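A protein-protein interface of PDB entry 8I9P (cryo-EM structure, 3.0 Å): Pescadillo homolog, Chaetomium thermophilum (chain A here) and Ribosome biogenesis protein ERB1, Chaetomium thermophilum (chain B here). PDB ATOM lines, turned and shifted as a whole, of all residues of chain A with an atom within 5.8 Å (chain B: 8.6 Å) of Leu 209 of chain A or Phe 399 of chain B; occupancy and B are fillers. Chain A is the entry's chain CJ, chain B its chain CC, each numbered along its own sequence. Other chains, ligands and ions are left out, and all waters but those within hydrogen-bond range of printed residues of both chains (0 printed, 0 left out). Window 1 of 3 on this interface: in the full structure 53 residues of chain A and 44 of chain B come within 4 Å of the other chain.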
ATOM      1  N   LEU A 145      -1.665 -13.524  36.002  1.00  0.00           N
ATOM      2  CA  LEU A 145      -2.720 -14.322  35.401  1.00  0.00           C
ATOM      3  C   LEU A 145      -2.651 -14.303  33.881  1.00  0.00           C
ATOM      4  O   LEU A 145      -2.967 -15.317  33.242  1.00  0.00           O
ATOM      5  CB  LEU A 145      -4.057 -13.784  35.893  1.00  0.00           C
ATOM      6  CG  LEU A 145      -5.386 -14.301  35.386  1.00  0.00           C
ATOM      7  CD1 LEU A 145      -5.570 -15.748  35.801  1.00  0.00           C
ATOM      8  CD2 LEU A 145      -6.420 -13.400  35.998  1.00  0.00           C
ATOM      9  N   SER A 146      -2.224 -13.177  33.289  1.00  0.00           N
ATOM     10  CA  SER A 146      -1.988 -13.158  31.847  1.00  0.00           C
ATOM     11  C   SER A 146      -0.894 -14.151  31.447  1.00  0.00           C
ATOM     12  O   SER A 146      -1.070 -14.944  30.499  1.00  0.00           O
ATOM     13  CB  SER A 146      -1.622 -11.744  31.403  1.00  0.00           C
ATOM     14  OG  SER A 146      -2.418 -10.786  32.074  1.00  0.00           O
ATOM     15  N   PHE A 149      -2.322 -17.863  31.897  1.00  0.00           N
ATOM     16  CA  PHE A 149      -3.240 -18.311  30.854  1.00  0.00           C
ATOM     17  C   PHE A 149      -2.504 -18.616  29.556  1.00  0.00           C
ATOM     18  O   PHE A 149      -2.762 -19.658  28.923  1.00  0.00           O
ATOM     19  CB  PHE A 149      -4.343 -17.277  30.633  1.00  0.00           C
ATOM     20  CG  PHE A 149      -5.637 -17.645  31.286  1.00  0.00           C
ATOM     21  CD1 PHE A 149      -6.351 -18.747  30.847  1.00  0.00           C
ATOM     22  CD2 PHE A 149      -6.108 -16.933  32.374  1.00  0.00           C
ATOM     23  CE1 PHE A 149      -7.532 -19.103  31.452  1.00  0.00           C
ATOM     24  CE2 PHE A 149      -7.285 -17.295  32.992  1.00  0.00           C
ATOM     25  CZ  PHE A 149      -7.999 -18.374  32.526  1.00  0.00           C
ATOM     26  N   LEU A 150      -1.549 -17.754  29.166  1.00  0.00           N
ATOM     27  CA  LEU A 150      -0.759 -18.071  27.974  1.00  0.00           C
ATOM     28  C   LEU A 150       0.037 -19.360  28.170  1.00  0.00           C
ATOM     29  O   LEU A 150       0.088 -20.216  27.277  1.00  0.00           O
ATOM     30  CB  LEU A 150       0.188 -16.923  27.619  1.00  0.00           C
ATOM     31  CG  LEU A 150       1.386 -17.393  26.776  1.00  0.00           C
ATOM     32  CD1 LEU A 150       0.969 -17.568  25.310  1.00  0.00           C
ATOM     33  CD2 LEU A 150       2.626 -16.549  26.917  1.00  0.00           C
ATOM     34  N   SER A 191     -10.667 -10.348  20.261  1.00  0.00           N
ATOM     35  CA  SER A 191      -9.884  -9.703  19.211  1.00  0.00           C
ATOM     36  C   SER A 191      -8.934 -10.649  18.477  1.00  0.00           C
ATOM     37  O   SER A 191      -9.092 -11.868  18.538  1.00  0.00           O
ATOM     38  CB  SER A 191      -9.084  -8.563  19.822  1.00  0.00           C
ATOM     39  OG  SER A 191      -8.435  -8.973  21.016  1.00  0.00           O
ATOM     40  N   ILE A 192      -7.948 -10.085  17.770  1.00  0.00           N
ATOM     41  CA  ILE A 192      -6.962 -10.904  17.065  1.00  0.00           C
ATOM     42  C   ILE A 192      -5.734 -11.188  17.929  1.00  0.00           C
ATOM     43  O   ILE A 192      -4.955 -12.097  17.622  1.00  0.00           O
ATOM     44  CB  ILE A 192      -6.607 -10.285  15.692  1.00  0.00           C
ATOM     45  CG1 ILE A 192      -7.775 -10.274  14.687  1.00  0.00           C
ATOM     46  CG2 ILE A 192      -5.425 -11.020  15.097  1.00  0.00           C
ATOM     47  CD1 ILE A 192      -7.617  -9.466  13.405  1.00  0.00           C
ATOM     48  N   LYS A 193      -5.521 -10.404  18.990  1.00  0.00           N
ATOM     49  CA  LYS A 193      -4.770 -10.903  20.141  1.00  0.00           C
ATOM     50  C   LYS A 193      -5.373 -12.200  20.651  1.00  0.00           C
ATOM     51  O   LYS A 193      -4.678 -13.211  20.797  1.00  0.00           O
ATOM     52  CB  LYS A 193      -4.758  -9.854  21.262  1.00  0.00           C
ATOM     53  CG  LYS A 193      -3.889  -8.552  21.148  1.00  0.00           C
ATOM     54  CD  LYS A 193      -2.577  -8.470  20.333  1.00  0.00           C
ATOM     55  CE  LYS A 193      -1.566  -9.626  20.511  1.00  0.00           C
ATOM     56  NZ  LYS A 193      -0.207  -9.344  19.951  1.00  0.00           N
ATOM     57  N   GLY A 194      -6.675 -12.192  20.890  1.00  0.00           N
ATOM     58  CA  GLY A 194      -7.318 -13.190  21.727  1.00  0.00           C
ATOM     59  C   GLY A 194      -8.513 -12.540  22.379  1.00  0.00           C
ATOM     60  O   GLY A 194      -9.282 -11.831  21.722  1.00  0.00           O
ATOM     61  N   ILE A 195      -8.653 -12.766  23.683  1.00  0.00           N
ATOM     62  CA  ILE A 195      -9.696 -12.125  24.476  1.00  0.00           C
ATOM     63  C   ILE A 195      -9.058 -11.479  25.698  1.00  0.00           C
ATOM     64  O   ILE A 195      -8.332 -12.140  26.450  1.00  0.00           O
ATOM     65  CB  ILE A 195     -10.801 -13.109  24.900  1.00  0.00           C
ATOM     66  CG1 ILE A 195     -11.184 -14.053  23.750  1.00  0.00           C
ATOM     67  CG2 ILE A 195     -11.993 -12.327  25.403  1.00  0.00           C
ATOM     68  CD1 ILE A 195     -12.478 -14.791  23.944  1.00  0.00           C
ATOM     69  N   TYR A 196      -9.320 -10.186  25.889  1.00  0.00           N
ATOM     70  CA  TYR A 196      -9.053  -9.517  27.152  1.00  0.00           C
ATOM     71  C   TYR A 196     -10.287  -9.637  28.038  1.00  0.00           C
ATOM     72  O   TYR A 196     -11.425  -9.605  27.555  1.00  0.00           O
ATOM     73  CB  TYR A 196      -8.717  -8.025  26.987  1.00  0.00           C
ATOM     74  CG  TYR A 196      -7.444  -7.634  26.242  1.00  0.00           C
ATOM     75  CD1 TYR A 196      -7.117  -8.184  25.010  1.00  0.00           C
ATOM     76  CD2 TYR A 196      -6.645  -6.596  26.715  1.00  0.00           C
ATOM     77  CE1 TYR A 196      -5.982  -7.788  24.324  1.00  0.00           C
ATOM     78  CE2 TYR A 196      -5.501  -6.197  26.042  1.00  0.00           C
ATOM     79  CZ  TYR A 196      -5.179  -6.793  24.845  1.00  0.00           C
ATOM     80  OH  TYR A 196      -4.051  -6.393  24.165  1.00  0.00           O
ATOM     81  N   TYR A 197     -10.056  -9.764  29.338  1.00  0.00           N
ATOM     82  CA  TYR A 197     -11.114  -9.789  30.333  1.00  0.00           C
ATOM     83  C   TYR A 197     -10.771  -8.806  31.441  1.00  0.00           C
ATOM     84  O   TYR A 197      -9.620  -8.738  31.884  1.00  0.00           O
ATOM     85  CB  TYR A 197     -11.292 -11.188  30.929  1.00  0.00           C
ATOM     86  CG  TYR A 197     -11.538 -12.312  29.942  1.00  0.00           C
ATOM     87  CD1 TYR A 197     -10.479 -12.957  29.315  1.00  0.00           C
ATOM     88  CD2 TYR A 197     -12.825 -12.726  29.637  1.00  0.00           C
ATOM     89  CE1 TYR A 197     -10.692 -13.991  28.429  1.00  0.00           C
ATOM     90  CE2 TYR A 197     -13.048 -13.759  28.745  1.00  0.00           C
ATOM     91  CZ  TYR A 197     -11.979 -14.389  28.147  1.00  0.00           C
ATOM     92  OH  TYR A 197     -12.197 -15.411  27.251  1.00  0.00           O
ATOM     93  N   LEU A 207      -7.095  -6.640  34.275  1.00  0.00           N
ATOM     94  CA  LEU A 207      -7.195  -6.909  32.847  1.00  0.00           C
ATOM     95  C   LEU A 207      -6.232  -8.032  32.494  1.00  0.00           C
ATOM     96  O   LEU A 207      -5.060  -7.987  32.876  1.00  0.00           O
ATOM     97  CB  LEU A 207      -6.864  -5.658  32.026  1.00  0.00           C
ATOM     98  CG  LEU A 207      -7.959  -4.612  31.817  1.00  0.00           C
ATOM     99  CD1 LEU A 207      -7.343  -3.242  31.592  1.00  0.00           C
ATOM    100  CD2 LEU A 207      -8.822  -4.999  30.630  1.00  0.00           C
ATOM    101  N   TRP A 208      -6.713  -9.031  31.760  1.00  0.00           N
ATOM    102  CA  TRP A 208      -5.862 -10.181  31.482  1.00  0.00           C
ATOM    103  C   TRP A 208      -6.293 -10.842  30.181  1.00  0.00           C
ATOM    104  O   TRP A 208      -7.486 -10.945  29.881  1.00  0.00           O
ATOM    105  CB  TRP A 208      -5.883 -11.158  32.665  1.00  0.00           C
ATOM    106  CG  TRP A 208      -7.251 -11.495  33.152  1.00  0.00           C
ATOM    107  CD1 TRP A 208      -7.951 -10.859  34.136  1.00  0.00           C
ATOM    108  CD2 TRP A 208      -8.039 -12.626  32.770  1.00  0.00           C
ATOM    109  NE1 TRP A 208      -9.157 -11.484  34.338  1.00  0.00           N
ATOM    110  CE2 TRP A 208      -9.231 -12.578  33.518  1.00  0.00           C
ATOM    111  CE3 TRP A 208      -7.863 -13.661  31.848  1.00  0.00           C
ATOM    112  CZ2 TRP A 208     -10.243 -13.522  33.369  1.00  0.00           C
ATOM    113  CZ3 TRP A 208      -8.865 -14.601  31.711  1.00  0.00           C
ATOM    114  CH2 TRP A 208     -10.041 -14.524  32.463  1.00  0.00           C
ATOM    115  N   LEU A 209      -5.302 -11.292  29.416  1.00  0.00           N
ATOM    116  CA  LEU A 209      -5.465 -11.658  28.016  1.00  0.00           C
ATOM    117  C   LEU A 209      -5.172 -13.138  27.801  1.00  0.00           C
ATOM    118  O   LEU A 209      -4.186 -13.670  28.321  1.00  0.00           O
ATOM    119  CB  LEU A 209      -4.545 -10.794  27.146  1.00  0.00           C
ATOM    120  CG  LEU A 209      -4.261 -11.131  25.682  1.00  0.00           C
ATOM    121  CD1 LEU A 209      -5.511 -11.315  24.826  1.00  0.00           C
ATOM    122  CD2 LEU A 209      -3.336 -10.075  25.086  1.00  0.00           C
ATOM    123  N   VAL A 210      -6.033 -13.789  27.026  1.00  0.00           N
ATOM    124  CA  VAL A 210      -5.911 -15.204  26.693  1.00  0.00           C
ATOM    125  C   VAL A 210      -5.861 -15.328  25.177  1.00  0.00           C
ATOM    126  O   VAL A 210      -6.700 -14.740  24.491  1.00  0.00           O
ATOM    127  CB  VAL A 210      -7.075 -16.042  27.254  1.00  0.00           C
ATOM    128  CG1 VAL A 210      -6.852 -17.522  26.989  1.00  0.00           C
ATOM    129  CG2 VAL A 210      -7.243 -15.795  28.741  1.00  0.00           C
ATOM    130  N   PRO A 211      -4.908 -16.065  24.612  1.00  0.00           N
ATOM    131  CA  PRO A 211      -4.944 -16.355  23.177  1.00  0.00           C
ATOM    132  C   PRO A 211      -5.849 -17.539  22.864  1.00  0.00           C
ATOM    133  O   PRO A 211      -6.335 -18.242  23.751  1.00  0.00           O
ATOM    134  CB  PRO A 211      -3.483 -16.675  22.851  1.00  0.00           C
ATOM    135  CG  PRO A 211      -2.962 -17.280  24.113  1.00  0.00           C
ATOM    136  CD  PRO A 211      -3.709 -16.628  25.257  1.00  0.00           C
ATOM    137  N   GLN A 216       0.940 -22.137  18.644  1.00  0.00           N
ATOM    138  CA  GLN A 216       1.727 -20.911  18.677  1.00  0.00           C
ATOM    139  C   GLN A 216       3.194 -21.241  18.436  1.00  0.00           C
ATOM    140  O   GLN A 216       3.776 -22.063  19.150  1.00  0.00           O
ATOM    141  CB  GLN A 216       1.570 -20.184  20.014  1.00  0.00           C
ATOM    142  CG  GLN A 216       0.201 -19.571  20.245  1.00  0.00           C
ATOM    143  CD  GLN A 216      -0.648 -20.391  21.192  1.00  0.00           C
ATOM    144  OE1 GLN A 216      -0.220 -21.438  21.678  1.00  0.00           O
ATOM    145  NE2 GLN A 216      -1.860 -19.920  21.463  1.00  0.00           N
ATOM    146  N   LEU B 345      -0.974  -1.917  32.107  1.00  0.00           N
ATOM    147  CA  LEU B 345      -1.151  -1.905  30.663  1.00  0.00           C
ATOM    148  C   LEU B 345      -2.301  -0.976  30.281  1.00  0.00           C
ATOM    149  O   LEU B 345      -3.259  -0.828  31.048  1.00  0.00           O
ATOM    150  CB  LEU B 345      -1.419  -3.320  30.149  1.00  0.00           C
ATOM    151  CG  LEU B 345      -0.215  -4.262  30.165  1.00  0.00           C
ATOM    152  CD1 LEU B 345      -0.614  -5.662  29.723  1.00  0.00           C
ATOM    153  CD2 LEU B 345       0.904  -3.715  29.290  1.00  0.00           C
ATOM    154  N   PRO B 348      -7.839  -1.464  26.308  1.00  0.00           N
ATOM    155  CA  PRO B 348      -7.979  -1.722  24.863  1.00  0.00           C
ATOM    156  C   PRO B 348      -8.764  -0.615  24.174  1.00  0.00           C
ATOM    157  O   PRO B 348      -9.853  -0.240  24.614  1.00  0.00           O
ATOM    158  CB  PRO B 348      -8.731  -3.059  24.812  1.00  0.00           C
ATOM    159  CG  PRO B 348      -8.543  -3.665  26.159  1.00  0.00           C
ATOM    160  CD  PRO B 348      -8.462  -2.524  27.117  1.00  0.00           C
ATOM    161  N   LEU B 352      -9.016  -2.102  18.019  1.00  0.00           N
ATOM    162  CA  LEU B 352      -8.549  -3.476  18.159  1.00  0.00           C
ATOM    163  C   LEU B 352      -9.692  -4.487  18.200  1.00  0.00           C
ATOM    164  O   LEU B 352      -9.492  -5.621  18.634  1.00  0.00           O
ATOM    165  CB  LEU B 352      -7.615  -3.518  19.385  1.00  0.00           C
ATOM    166  CG  LEU B 352      -6.522  -4.508  19.833  1.00  0.00           C
ATOM    167  CD1 LEU B 352      -6.966  -5.790  20.449  1.00  0.00           C
ATOM    168  CD2 LEU B 352      -5.820  -4.915  18.571  1.00  0.00           C
ATOM    169  N   ALA B 395      -5.187 -17.168  15.169  1.00  0.00           N
ATOM    170  CA  ALA B 395      -4.400 -16.773  16.326  1.00  0.00           C
ATOM    171  C   ALA B 395      -3.027 -16.277  15.896  1.00  0.00           C
ATOM    172  O   ALA B 395      -2.322 -16.923  15.117  1.00  0.00           O
ATOM    173  CB  ALA B 395      -4.249 -17.939  17.305  1.00  0.00           C
ATOM    174  N   TRP B 396      -2.661 -15.108  16.403  1.00  0.00           N
ATOM    175  CA  TRP B 396      -1.379 -14.506  16.079  1.00  0.00           C
ATOM    176  C   TRP B 396      -0.353 -15.017  17.093  1.00  0.00           C
ATOM    177  O   TRP B 396      -0.599 -14.991  18.298  1.00  0.00           O
ATOM    178  CB  TRP B 396      -1.567 -12.974  16.045  1.00  0.00           C
ATOM    179  CG  TRP B 396      -0.421 -11.984  16.286  1.00  0.00           C
ATOM    180  CD1 TRP B 396       0.929 -12.221  16.248  1.00  0.00           C
ATOM    181  CD2 TRP B 396      -0.565 -10.564  16.547  1.00  0.00           C
ATOM    182  NE1 TRP B 396       1.611 -11.052  16.499  1.00  0.00           N
ATOM    183  CE2 TRP B 396       0.715 -10.031  16.684  1.00  0.00           C
ATOM    184  CE3 TRP B 396      -1.669  -9.698  16.684  1.00  0.00           C
ATOM    185  CZ2 TRP B 396       0.924  -8.679  16.923  1.00  0.00           C
ATOM    186  CZ3 TRP B 396      -1.452  -8.369  16.947  1.00  0.00           C
ATOM    187  CH2 TRP B 396      -0.181  -7.865  17.023  1.00  0.00           C
ATOM    188  N   GLY B 397       0.761 -15.561  16.588  1.00  0.00           N
ATOM    189  CA  GLY B 397       1.626 -16.387  17.425  1.00  0.00           C
ATOM    190  C   GLY B 397       2.711 -15.597  18.133  1.00  0.00           C
ATOM    191  O   GLY B 397       3.085 -15.908  19.273  1.00  0.00           O
ATOM    192  N   ASN B 398       3.182 -14.521  17.496  1.00  0.00           N
ATOM    193  CA  ASN B 398       4.127 -13.553  18.044  1.00  0.00           C
ATOM    194  C   ASN B 398       3.587 -12.909  19.335  1.00  0.00           C
ATOM    195  O   ASN B 398       4.357 -12.274  20.069  1.00  0.00           O
ATOM    196  CB  ASN B 398       4.437 -12.513  16.954  1.00  0.00           C
ATOM    197  CG  ASN B 398       5.696 -11.680  17.204  1.00  0.00           C
ATOM    198  OD1 ASN B 398       6.230 -11.595  18.300  1.00  0.00           O
ATOM    199  ND2 ASN B 398       6.176 -11.051  16.137  1.00  0.00           N
ATOM    200  N   PHE B 399       2.282 -13.105  19.609  1.00  0.00           N
ATOM    201  CA  PHE B 399       1.692 -12.984  20.942  1.00  0.00           C
ATOM    202  C   PHE B 399       2.676 -13.377  22.025  1.00  0.00           C
ATOM    203  O   PHE B 399       3.109 -12.513  22.800  1.00  0.00           O
ATOM    204  CB  PHE B 399       0.461 -13.898  20.994  1.00  0.00           C
ATOM    205  CG  PHE B 399      -0.426 -13.745  22.204  1.00  0.00           C
ATOM    206  CD1 PHE B 399      -0.084 -14.332  23.418  1.00  0.00           C
ATOM    207  CD2 PHE B 399      -1.641 -13.092  22.106  1.00  0.00           C
ATOM    208  CE1 PHE B 399      -0.901 -14.225  24.514  1.00  0.00           C
ATOM    209  CE2 PHE B 399      -2.466 -12.987  23.204  1.00  0.00           C
ATOM    210  CZ  PHE B 399      -2.092 -13.555  24.408  1.00  0.00           C
ATOM    211  N   VAL B 400       3.159 -14.630  21.982  1.00  0.00           N
ATOM    212  CA  VAL B 400       4.048 -15.134  23.027  1.00  0.00           C
ATOM    213  C   VAL B 400       5.265 -14.236  23.144  1.00  0.00           C
ATOM    214  O   VAL B 400       5.515 -13.653  24.212  1.00  0.00           O
ATOM    215  CB  VAL B 400       4.461 -16.590  22.741  1.00  0.00           C
ATOM    216  CG1 VAL B 400       5.238 -17.164  23.924  1.00  0.00           C
ATOM    217  CG2 VAL B 400       3.247 -17.444  22.413  1.00  0.00           C
ATOM    218  N   LYS B 401       5.912 -13.957  22.005  1.00  0.00           N
ATOM    219  CA  LYS B 401       7.117 -13.143  22.024  1.00  0.00           C
ATOM    220  C   LYS B 401       6.825 -11.730  22.499  1.00  0.00           C
ATOM    221  O   LYS B 401       7.548 -11.211  23.361  1.00  0.00           O
ATOM    222  CB  LYS B 401       7.778 -13.116  20.644  1.00  0.00           C
ATOM    223  CG  LYS B 401       7.777 -14.426  19.879  1.00  0.00           C
ATOM    224  CD  LYS B 401       8.353 -14.204  18.483  1.00  0.00           C
ATOM    225  CE  LYS B 401       7.752 -15.164  17.471  1.00  0.00           C
ATOM    226  NZ  LYS B 401       8.051 -14.778  16.064  1.00  0.00           N
ATOM    227  N   GLU B 402       5.723 -11.117  22.028  1.00  0.00           N
ATOM    228  CA  GLU B 402       5.483  -9.746  22.484  1.00  0.00           C
ATOM    229  C   GLU B 402       5.075  -9.768  23.942  1.00  0.00           C
ATOM    230  O   GLU B 402       5.482  -8.897  24.720  1.00  0.00           O
ATOM    231  CB  GLU B 402       4.435  -9.010  21.632  1.00  0.00           C
ATOM    232  CG  GLU B 402       3.055  -9.618  21.418  1.00  0.00           C
ATOM    233  CD  GLU B 402       2.120  -9.431  22.615  1.00  0.00           C
ATOM    234  OE1 GLU B 402       2.228  -8.390  23.303  1.00  0.00           O
ATOM    235  OE2 GLU B 402       1.273 -10.315  22.868  1.00  0.00           O
ATOM    236  N   ARG B 403       4.353 -10.822  24.340  1.00  0.00           N
ATOM    237  CA  ARG B 403       4.086 -11.014  25.752  1.00  0.00           C
ATOM    238  C   ARG B 403       5.411 -11.194  26.476  1.00  0.00           C
ATOM    239  O   ARG B 403       5.706 -10.459  27.425  1.00  0.00           O
ATOM    240  CB  ARG B 403       3.132 -12.212  25.918  1.00  0.00           C
ATOM    241  CG  ARG B 403       3.165 -13.070  27.194  1.00  0.00           C
ATOM    242  CD  ARG B 403       3.115 -12.330  28.503  1.00  0.00           C
ATOM    243  NE  ARG B 403       2.242 -11.140  28.518  1.00  0.00           N
ATOM    244  CZ  ARG B 403       0.919 -11.160  28.481  1.00  0.00           C
ATOM    245  NH1 ARG B 403       0.241 -12.300  28.471  1.00  0.00           N
ATOM    246  NH2 ARG B 403       0.267 -10.012  28.468  1.00  0.00           N
ATOM    247  N   PHE B 404       6.275 -12.065  25.928  1.00  0.00           N
ATOM    248  CA  PHE B 404       7.630 -12.232  26.442  1.00  0.00           C
ATOM    249  C   PHE B 404       8.362 -10.901  26.475  1.00  0.00           C
ATOM    250  O   PHE B 404       9.011 -10.578  27.481  1.00  0.00           O
ATOM    251  CB  PHE B 404       8.398 -13.241  25.593  1.00  0.00           C
ATOM    252  CG  PHE B 404       9.789 -13.522  26.090  1.00  0.00           C
ATOM    253  CD1 PHE B 404      10.023 -13.771  27.432  1.00  0.00           C
ATOM    254  CD2 PHE B 404      10.859 -13.553  25.206  1.00  0.00           C
ATOM    255  CE1 PHE B 404      11.301 -14.038  27.883  1.00  0.00           C
ATOM    256  CE2 PHE B 404      12.137 -13.818  25.654  1.00  0.00           C
ATOM    257  CZ  PHE B 404      12.357 -14.060  26.993  1.00  0.00           C
ATOM    258  N   GLU B 405       8.157 -10.080  25.427  1.00  0.00           N
ATOM    259  CA  GLU B 405       8.784  -8.765  25.349  1.00  0.00           C
ATOM    260  C   GLU B 405       8.451  -7.938  26.579  1.00  0.00           C
ATOM    261  O   GLU B 405       9.362  -7.499  27.304  1.00  0.00           O
ATOM    262  CB  GLU B 405       8.340  -8.038  24.077  1.00  0.00           C
ATOM    263  CG  GLU B 405       9.165  -8.325  22.827  1.00  0.00           C
ATOM    264  CD  GLU B 405      10.288  -7.320  22.593  1.00  0.00           C
ATOM    265  OE1 GLU B 405      10.620  -6.549  23.519  1.00  0.00           O
ATOM    266  OE2 GLU B 405      10.820  -7.287  21.462  1.00  0.00           O
ATOM    267  N   ARG B 406       7.161  -7.853  26.921  1.00  0.00           N
ATOM    268  CA  ARG B 406       6.810  -6.947  28.000  1.00  0.00           C
ATOM    269  C   ARG B 406       7.334  -7.451  29.334  1.00  0.00           C
ATOM    270  O   ARG B 406       7.644  -6.621  30.197  1.00  0.00           O
ATOM    271  CB  ARG B 406       5.299  -6.694  28.066  1.00  0.00           C
ATOM    272  CG  ARG B 406       4.449  -7.796  28.654  1.00  0.00           C
ATOM    273  CD  ARG B 406       3.043  -7.286  28.937  1.00  0.00           C
ATOM    274  NE  ARG B 406       2.585  -6.366  27.903  1.00  0.00           N
ATOM    275  CZ  ARG B 406       1.955  -6.742  26.799  1.00  0.00           C
ATOM    276  NH1 ARG B 406       1.683  -8.014  26.559  1.00  0.00           N
ATOM    277  NH2 ARG B 406       1.597  -5.820  25.910  1.00  0.00           N
ATOM    278  N   CYS B 407       7.558  -8.776  29.471  1.00  0.00           N
ATOM    279  CA  CYS B 407       8.105  -9.281  30.730  1.00  0.00           C
ATOM    280  C   CYS B 407       9.467  -8.676  31.022  1.00  0.00           C
ATOM    281  O   CYS B 407       9.664  -8.117  32.113  1.00  0.00           O
ATOM    282  CB  CYS B 407       8.184 -10.810  30.773  1.00  0.00           C
ATOM    283  SG  CYS B 407       6.948 -11.764  29.902  1.00  0.00           S
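The side-chain amino group (NZ) of Lys 193 of chain A is in salt-bridge range of the side-chain carboxylate (OE2) of Glu 402 of chain B, at 3.4 Å.
The side-chain sulfur of Cys 407 of chain B lies within hydrogen-bond range of the backbone carbonyl oxygen of Arg 403 of chain B.
The side-chain carboxylate (OE1) of Glu 402 of chain B is in salt-bridge range of the guanidinium group (NH1) of Arg 406 of chain B (3.3 Å).
The side-chain hydroxyl of Ser 191 of chain A sits at hydrogen-bond distance from the backbone carbonyl oxygen of Gly 194 of chain A, at 3.1 Å.
Among the printed residues, merely in contact across the chains: Ser 191 of chain A with Leu 352 of chain B (3.2 Å), Lys 193 of chain A with Phe 399 of chain B (3.3 Å), Lys 193 of chain A with Trp 396 of chain B (3.3 Å), Leu 209 of chain A with Phe 399 of chain B (3.5 Å), Ser 146 of chain A with Arg 403 of chain B (3.5 Å), Leu 150 of chain A with Arg 403 of chain B (3.5 Å), Tyr 196 of chain A with Pro 348 of chain B (3.5 Å), Pro 211 of chain A with Phe 399 of chain B (3.6 Å), Leu 150 of chain A with Val 400 of chain B (3.7 Å), Ile 192 of chain A with Trp 396 of chain B (3.8 Å) and Leu 150 of chain A with Phe 399 of chain B (3.9 Å).
Of chain B, only Phe 399 (3.5 Å) comes within 4 Å of Leu 209 of chain A.
Of chain A, only Leu 150, Lys 193, Leu 209 and Pro 211 come within 4 Å of Phe 399 of chain B.
Of the printed residues of chain A, Pro 348 of chain B touches Tyr 196 (3.5 Å).
Of the printed residues of chain B, Ile 192 of chain A touches Trp 396 (3.8 Å).
Cys 407 of chain B touches none of the printed residues of chain A.
The nearest residue of chain A that does not touch Phe 399 of chain B is Val 210 of chain A (4.2 Å).
The nearest printed residue of chain B that does not touch Tyr 196 of chain A is Leu 352 of chain B (4.5 Å).
Of the 17 printed residues of chain A, 8 touch a printed residue of chain B.
Hydrophobic or aromatic side chains of chain A that line the printed part of chain B: Leu 150, Tyr 196, Leu 209 and Pro 211.
Printed residues of chain B that touch a printed residue of chain A: Pro 348, Leu 352, Trp 396, Phe 399, Val 400, Glu 402 and Arg 403.
Hydrophobic or aromatic side chains of chain B that line the printed part of chain A: Pro 348, Leu 352, Trp 396, Phe 399 and Val 400.
Among the printed residues, Asp or Glu carboxylates within 4 Å of a Lys or Arg side-chain nitrogen of the other chain: Lys 193 of chain A with Glu 402 of chain B (3.4 Å).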
